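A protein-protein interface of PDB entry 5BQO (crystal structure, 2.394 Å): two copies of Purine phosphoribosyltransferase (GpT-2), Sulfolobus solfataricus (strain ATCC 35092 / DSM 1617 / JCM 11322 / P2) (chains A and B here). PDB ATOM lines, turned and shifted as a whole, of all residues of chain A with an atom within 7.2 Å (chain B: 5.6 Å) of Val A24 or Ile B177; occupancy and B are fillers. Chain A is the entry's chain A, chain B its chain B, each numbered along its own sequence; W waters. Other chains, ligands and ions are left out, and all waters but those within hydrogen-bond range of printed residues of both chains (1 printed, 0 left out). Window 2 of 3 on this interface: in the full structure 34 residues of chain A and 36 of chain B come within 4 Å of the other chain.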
ATOM      1  N   SER A  18      14.990   7.108   8.088  1.00  0.00           N
ATOM      2  CA  SER A  18      15.956   7.928   8.812  1.00  0.00           C
ATOM      3  C   SER A  18      16.864   7.089   9.706  1.00  0.00           C
ATOM      4  O   SER A  18      18.078   7.291   9.736  1.00  0.00           O
ATOM      5  CB  SER A  18      15.230   8.981   9.650  1.00  0.00           C
ATOM      6  OG  SER A  18      16.144   9.739  10.421  1.00  0.00           O
ATOM      7  N   ILE A  19      16.265   6.152  10.434  1.00  0.00           N
ATOM      8  CA  ILE A  19      17.018   5.259  11.304  1.00  0.00           C
ATOM      9  C   ILE A  19      17.916   4.345  10.475  1.00  0.00           C
ATOM     10  O   ILE A  19      19.065   4.090  10.838  1.00  0.00           O
ATOM     11  CB  ILE A  19      16.079   4.412  12.187  1.00  0.00           C
ATOM     12  CG1 ILE A  19      15.338   5.309  13.180  1.00  0.00           C
ATOM     13  CG2 ILE A  19      16.854   3.334  12.929  1.00  0.00           C
ATOM     14  CD1 ILE A  19      14.165   4.633  13.855  1.00  0.00           C
ATOM     15  N   GLY A  20      17.388   3.871   9.351  1.00  0.00           N
ATOM     16  CA  GLY A  20      18.139   3.015   8.452  1.00  0.00           C
ATOM     17  C   GLY A  20      19.375   3.701   7.904  1.00  0.00           C
ATOM     18  O   GLY A  20      20.473   3.145   7.950  1.00  0.00           O
ATOM     19  N   GLU A  21      19.196   4.913   7.387  1.00  0.00           N
ATOM     20  CA  GLU A  21      20.310   5.693   6.864  1.00  0.00           C
ATOM     21  C   GLU A  21      21.338   5.977   7.954  1.00  0.00           C
ATOM     22  O   GLU A  21      22.541   5.853   7.728  1.00  0.00           O
ATOM     23  CB  GLU A  21      19.811   7.005   6.253  1.00  0.00           C
ATOM     24  CG  GLU A  21      18.965   6.821   5.003  1.00  0.00           C
ATOM     25  CD  GLU A  21      18.314   8.110   4.542  1.00  0.00           C
ATOM     26  OE1 GLU A  21      18.498   9.145   5.216  1.00  0.00           O
ATOM     27  OE2 GLU A  21      17.617   8.089   3.505  1.00  0.00           O
ATOM     28  N   ALA A  22      20.853   6.345   9.137  1.00  0.00           N
ATOM     29  CA  ALA A  22      21.720   6.637  10.275  1.00  0.00           C
ATOM     30  C   ALA A  22      22.615   5.448  10.614  1.00  0.00           C
ATOM     31  O   ALA A  22      23.775   5.620  10.983  1.00  0.00           O
ATOM     32  CB  ALA A  22      20.888   7.035  11.487  1.00  0.00           C
ATOM     33  N   LEU A  23      22.069   4.244  10.475  1.00  0.00           N
ATOM     34  CA  LEU A  23      22.818   3.020  10.740  1.00  0.00           C
ATOM     35  C   LEU A  23      23.907   2.783   9.697  1.00  0.00           C
ATOM     36  O   LEU A  23      25.040   2.440  10.036  1.00  0.00           O
ATOM     37  CB  LEU A  23      21.873   1.816  10.785  1.00  0.00           C
ATOM     38  CG  LEU A  23      20.915   1.729  11.973  1.00  0.00           C
ATOM     39  CD1 LEU A  23      19.794   0.741  11.688  1.00  0.00           C
ATOM     40  CD2 LEU A  23      21.667   1.339  13.234  1.00  0.00           C
ATOM     41  N   VAL A  24      23.553   2.967   8.429  1.00  0.00           N
ATOM     42  CA  VAL A  24      24.477   2.736   7.324  1.00  0.00           C
ATOM     43  C   VAL A  24      25.633   3.734   7.347  1.00  0.00           C
ATOM     44  O   VAL A  24      26.775   3.384   7.044  1.00  0.00           O
ATOM     45  CB  VAL A  24      23.751   2.815   5.965  1.00  0.00           C
ATOM     46  CG1 VAL A  24      24.723   2.584   4.819  1.00  0.00           C
ATOM     47  CG2 VAL A  24      22.623   1.799   5.915  1.00  0.00           C
ATOM     48  N   LYS A  25      25.337   4.975   7.718  1.00  0.00           N
ATOM     49  CA  LYS A  25      26.361   6.011   7.790  1.00  0.00           C
ATOM     50  C   LYS A  25      27.196   5.913   9.066  1.00  0.00           C
ATOM     51  O   LYS A  25      28.272   6.504   9.155  1.00  0.00           O
ATOM     52  CB  LYS A  25      25.723   7.396   7.679  1.00  0.00           C
ATOM     53  CG  LYS A  25      24.881   7.583   6.427  1.00  0.00           C
ATOM     54  CD  LYS A  25      24.259   8.968   6.368  1.00  0.00           C
ATOM     55  CE  LYS A  25      23.729   9.405   7.724  1.00  0.00           C
ATOM     56  NZ  LYS A  25      23.061  10.733   7.637  1.00  0.00           N
ATOM     57  N   SER A  26      26.697   5.165  10.047  1.00  0.00           N
ATOM     58  CA  SER A  26      27.437   4.921  11.281  1.00  0.00           C
ATOM     59  C   SER A  26      28.197   3.602  11.203  1.00  0.00           C
ATOM     60  O   SER A  26      28.825   3.179  12.175  1.00  0.00           O
ATOM     61  CB  SER A  26      26.497   4.910  12.487  1.00  0.00           C
ATOM     62  OG  SER A  26      25.912   6.183  12.696  1.00  0.00           O
ATOM     63  N   ASN A  27      28.126   2.963  10.038  1.00  0.00           N
ATOM     64  CA  ASN A  27      28.767   1.672   9.792  1.00  0.00           C
ATOM     65  C   ASN A  27      28.368   0.608  10.810  1.00  0.00           C
ATOM     66  O   ASN A  27      29.204  -0.174  11.265  1.00  0.00           O
ATOM     67  CB  ASN A  27      30.289   1.826   9.772  1.00  0.00           C
ATOM     68  CG  ASN A  27      30.776   2.631   8.585  1.00  0.00           C
ATOM     69  OD1 ASN A  27      30.924   2.105   7.482  1.00  0.00           O
ATOM     70  ND2 ASN A  27      31.026   3.917   8.804  1.00  0.00           N
ATOM     71  N   TYR A  28      27.088   0.583  11.164  1.00  0.00           N
ATOM     72  CA  TYR A  28      26.578  -0.421  12.089  1.00  0.00           C
ATOM     73  C   TYR A  28      25.431  -1.206  11.466  1.00  0.00           C
ATOM     74  O   TYR A  28      24.262  -0.862  11.642  1.00  0.00           O
ATOM     75  CB  TYR A  28      26.123   0.227  13.397  1.00  0.00           C
ATOM     76  CG  TYR A  28      25.819  -0.775  14.487  1.00  0.00           C
ATOM     77  CD1 TYR A  28      26.846  -1.414  15.171  1.00  0.00           C
ATOM     78  CD2 TYR A  28      24.510  -1.087  14.828  1.00  0.00           C
ATOM     79  CE1 TYR A  28      26.576  -2.335  16.165  1.00  0.00           C
ATOM     80  CE2 TYR A  28      24.231  -2.006  15.822  1.00  0.00           C
ATOM     81  CZ  TYR A  28      25.268  -2.627  16.486  1.00  0.00           C
ATOM     82  OH  TYR A  28      24.998  -3.542  17.478  1.00  0.00           O
ATOM     83  N   ILE A  29      25.775  -2.258  10.732  1.00  0.00           N
ATOM     84  CA  ILE A  29      24.777  -3.130  10.127  1.00  0.00           C
ATOM     85  C   ILE A  29      24.508  -4.316  11.045  1.00  0.00           C
ATOM     86  O   ILE A  29      25.349  -5.206  11.177  1.00  0.00           O
ATOM     87  CB  ILE A  29      25.224  -3.633   8.743  1.00  0.00           C
ATOM     88  CG1 ILE A  29      25.665  -2.456   7.868  1.00  0.00           C
ATOM     89  CG2 ILE A  29      24.109  -4.422   8.075  1.00  0.00           C
ATOM     90  CD1 ILE A  29      24.642  -1.342   7.778  1.00  0.00           C
ATOM     91  N   PRO A  30      23.330  -4.327  11.689  1.00  0.00           N
ATOM     92  CA  PRO A  30      22.974  -5.333  12.694  1.00  0.00           C
ATOM     93  C   PRO A  30      22.876  -6.741  12.119  1.00  0.00           C
ATOM     94  O   PRO A  30      22.314  -6.929  11.041  1.00  0.00           O
ATOM     95  CB  PRO A  30      21.602  -4.863  13.196  1.00  0.00           C
ATOM     96  CG  PRO A  30      21.494  -3.433  12.771  1.00  0.00           C
ATOM     97  CD  PRO A  30      22.248  -3.351  11.487  1.00  0.00           C
ATOM     98  N   LEU A  51      16.791  -2.759   5.156  1.00  0.00           N
ATOM     99  CA  LEU A  51      18.222  -3.043   5.176  1.00  0.00           C
ATOM    100  C   LEU A  51      18.534  -4.514   4.913  1.00  0.00           C
ATOM    101  O   LEU A  51      19.679  -4.946   5.065  1.00  0.00           O
ATOM    102  CB  LEU A  51      18.826  -2.618   6.519  1.00  0.00           C
ATOM    103  CG  LEU A  51      19.445  -1.220   6.614  1.00  0.00           C
ATOM    104  CD1 LEU A  51      18.570  -0.169   5.947  1.00  0.00           C
ATOM    105  CD2 LEU A  51      19.706  -0.853   8.067  1.00  0.00           C
ATOM    106  N   PHE A 134      19.798   5.458  18.304  1.00  0.00           N
ATOM    107  CA  PHE A 134      19.229   5.885  17.031  1.00  0.00           C
ATOM    108  C   PHE A 134      17.748   6.213  17.180  1.00  0.00           C
ATOM    109  O   PHE A 134      16.992   5.437  17.764  1.00  0.00           O
ATOM    110  CB  PHE A 134      19.416   4.804  15.963  1.00  0.00           C
ATOM    111  CG  PHE A 134      20.847   4.407  15.741  1.00  0.00           C
ATOM    112  CD1 PHE A 134      21.627   5.070  14.807  1.00  0.00           C
ATOM    113  CD2 PHE A 134      21.412   3.366  16.460  1.00  0.00           C
ATOM    114  CE1 PHE A 134      22.943   4.707  14.598  1.00  0.00           C
ATOM    115  CE2 PHE A 134      22.729   2.999  16.256  1.00  0.00           C
ATOM    116  CZ  PHE A 134      23.495   3.669  15.325  1.00  0.00           C
ATOM    117  N   LEU B 170      20.341   4.440  -0.634  1.00  0.00           N
ATOM    118  CA  LEU B 170      20.630   3.754   0.618  1.00  0.00           C
ATOM    119  C   LEU B 170      21.179   2.355   0.356  1.00  0.00           C
ATOM    120  O   LEU B 170      22.087   1.894   1.047  1.00  0.00           O
ATOM    121  CB  LEU B 170      19.370   3.674   1.480  1.00  0.00           C
ATOM    122  CG  LEU B 170      19.515   3.009   2.848  1.00  0.00           C
ATOM    123  CD1 LEU B 170      20.551   3.743   3.681  1.00  0.00           C
ATOM    124  CD2 LEU B 170      18.176   2.962   3.565  1.00  0.00           C
ATOM    125  N   GLN B 173      24.851   2.535  -0.829  1.00  0.00           N
ATOM    126  CA  GLN B 173      25.730   2.777   0.310  1.00  0.00           C
ATOM    127  C   GLN B 173      25.879   1.509   1.144  1.00  0.00           C
ATOM    128  O   GLN B 173      26.891   1.306   1.815  1.00  0.00           O
ATOM    129  CB  GLN B 173      25.190   3.911   1.183  1.00  0.00           C
ATOM    130  CG  GLN B 173      24.957   5.222   0.454  1.00  0.00           C
ATOM    131  CD  GLN B 173      24.276   6.257   1.330  1.00  0.00           C
ATOM    132  OE1 GLN B 173      23.123   6.621   1.100  1.00  0.00           O
ATOM    133  NE2 GLN B 173      24.989   6.734   2.344  1.00  0.00           N
ATOM    134  N   LEU B 174      24.856   0.661   1.092  1.00  0.00           N
ATOM    135  CA  LEU B 174      24.804  -0.550   1.901  1.00  0.00           C
ATOM    136  C   LEU B 174      25.674  -1.660   1.318  1.00  0.00           C
ATOM    137  O   LEU B 174      26.374  -2.359   2.050  1.00  0.00           O
ATOM    138  CB  LEU B 174      23.354  -1.026   2.034  1.00  0.00           C
ATOM    139  CG  LEU B 174      23.059  -2.121   3.059  1.00  0.00           C
ATOM    140  CD1 LEU B 174      23.867  -1.900   4.325  1.00  0.00           C
ATOM    141  CD2 LEU B 174      21.571  -2.163   3.377  1.00  0.00           C
ATOM    142  N   LEU B 175      25.625  -1.816  -0.001  1.00  0.00           N
ATOM    143  CA  LEU B 175      26.415  -2.834  -0.685  1.00  0.00           C
ATOM    144  C   LEU B 175      27.899  -2.479  -0.695  1.00  0.00           C
ATOM    145  O   LEU B 175      28.755  -3.351  -0.853  1.00  0.00           O
ATOM    146  CB  LEU B 175      25.914  -3.026  -2.118  1.00  0.00           C
ATOM    147  CG  LEU B 175      24.479  -3.537  -2.269  1.00  0.00           C
ATOM    148  CD1 LEU B 175      23.866  -3.068  -3.582  1.00  0.00           C
ATOM    149  CD2 LEU B 175      24.441  -5.054  -2.170  1.00  0.00           C
ATOM    150  N   LYS B 176      28.198  -1.196  -0.518  1.00  0.00           N
ATOM    151  CA  LYS B 176      29.576  -0.713  -0.547  1.00  0.00           C
ATOM    152  C   LYS B 176      30.324  -1.019   0.748  1.00  0.00           C
ATOM    153  O   LYS B 176      31.521  -0.745   0.856  1.00  0.00           O
ATOM    154  CB  LYS B 176      29.604   0.794  -0.817  1.00  0.00           C
ATOM    155  CG  LYS B 176      29.899   1.168  -2.263  1.00  0.00           C
ATOM    156  CD  LYS B 176      29.549   2.624  -2.545  1.00  0.00           C
ATOM    157  CE  LYS B 176      30.273   3.577  -1.604  1.00  0.00           C
ATOM    158  NZ  LYS B 176      30.216   4.986  -2.088  1.00  0.00           N
ATOM    159  N   ILE B 177      29.623  -1.580   1.730  1.00  0.00           N
ATOM    160  CA  ILE B 177      30.233  -1.887   3.023  1.00  0.00           C
ATOM    161  C   ILE B 177      29.879  -3.279   3.551  1.00  0.00           C
ATOM    162  O   ILE B 177      30.049  -3.555   4.738  1.00  0.00           O
ATOM    163  CB  ILE B 177      29.835  -0.849   4.097  1.00  0.00           C
ATOM    164  CG1 ILE B 177      28.318  -0.836   4.302  1.00  0.00           C
ATOM    165  CG2 ILE B 177      30.349   0.537   3.733  1.00  0.00           C
ATOM    166  CD1 ILE B 177      27.857   0.152   5.353  1.00  0.00           C
ATOM    167  N   ARG B 178      29.389  -4.154   2.678  1.00  0.00           N
ATOM    168  CA  ARG B 178      29.102  -5.528   3.082  1.00  0.00           C
ATOM    169  C   ARG B 178      30.170  -6.490   2.569  1.00  0.00           C
ATOM    170  O   ARG B 178      31.275  -6.077   2.217  1.00  0.00           O
ATOM    171  CB  ARG B 178      27.724  -5.970   2.588  1.00  0.00           C
ATOM    172  CG  ARG B 178      26.567  -5.438   3.416  1.00  0.00           C
ATOM    173  CD  ARG B 178      25.483  -6.490   3.582  1.00  0.00           C
ATOM    174  NE  ARG B 178      25.265  -7.256   2.358  1.00  0.00           N
ATOM    175  CZ  ARG B 178      24.083  -7.396   1.765  1.00  0.00           C
ATOM    176  NH1 ARG B 178      23.006  -6.821   2.284  1.00  0.00           N
ATOM    177  NH2 ARG B 178      23.977  -8.111   0.654  1.00  0.00           N
HETATM  178  O   HOH W   1      22.436  -6.248   4.727  1.00  0.00           O
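Val A24 touches just these residues of chain B: Leu B170, Gln B173 and Ile B177. Of the printed residues of chain A, Ile B177 touches Val A24. Printed residues of chain A within 4 Å of Gln B173: Val A24 (3.9 Å). Of the printed residues of chain B, Glu A21 touches Leu B170. Printed residues of chain A within 4 Å of Leu B170: Glu A21 (3.7 Å), Val A24 (3.6 Å) and Leu A51 (3.95 Å). Ser A18 touches none of the printed residues of chain B. The nearest residue of chain B that does not touch Val A24 is Leu B174 (4.2 Å). The nearest residue of chain A that does not touch Ile B177 is Asn A27 (4.1 Å). The nearest printed residue of chain A that does not touch Leu B170 is Gly A20 (4.3 Å).
Glu A21 touches Leu B170. Val A24 touches Leu B170 (CG2 to CD1, 3.6 Å). Val A24 touches Gln B173 (CG1 to CB, 3.9 Å). CD1 of Ile B177 touches O of Val A24, at 3.8 Å. Leu B174 touches Ile A29. Leu A51 touches Leu B170 (CD1 to CD2, 3.95 Å). Leu A51 touches Leu B174 (O to CD2, 3.8 Å).
Water W1 lies within hydrogen-bond range of NH1 of Arg B178 and O of Leu A51.
Of the 15 printed residues of chain A, 4 touch a printed residue of chain B. Hydrophobic or aromatic side chains of chain A that line the printed part of chain B: Val A24, Ile A29 and Leu A51. Of the 7 printed residues of chain B, 4 touch a printed residue of chain A. Among the printed residues, 7 pairs touch across the chains.
No position is printed for both chains.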
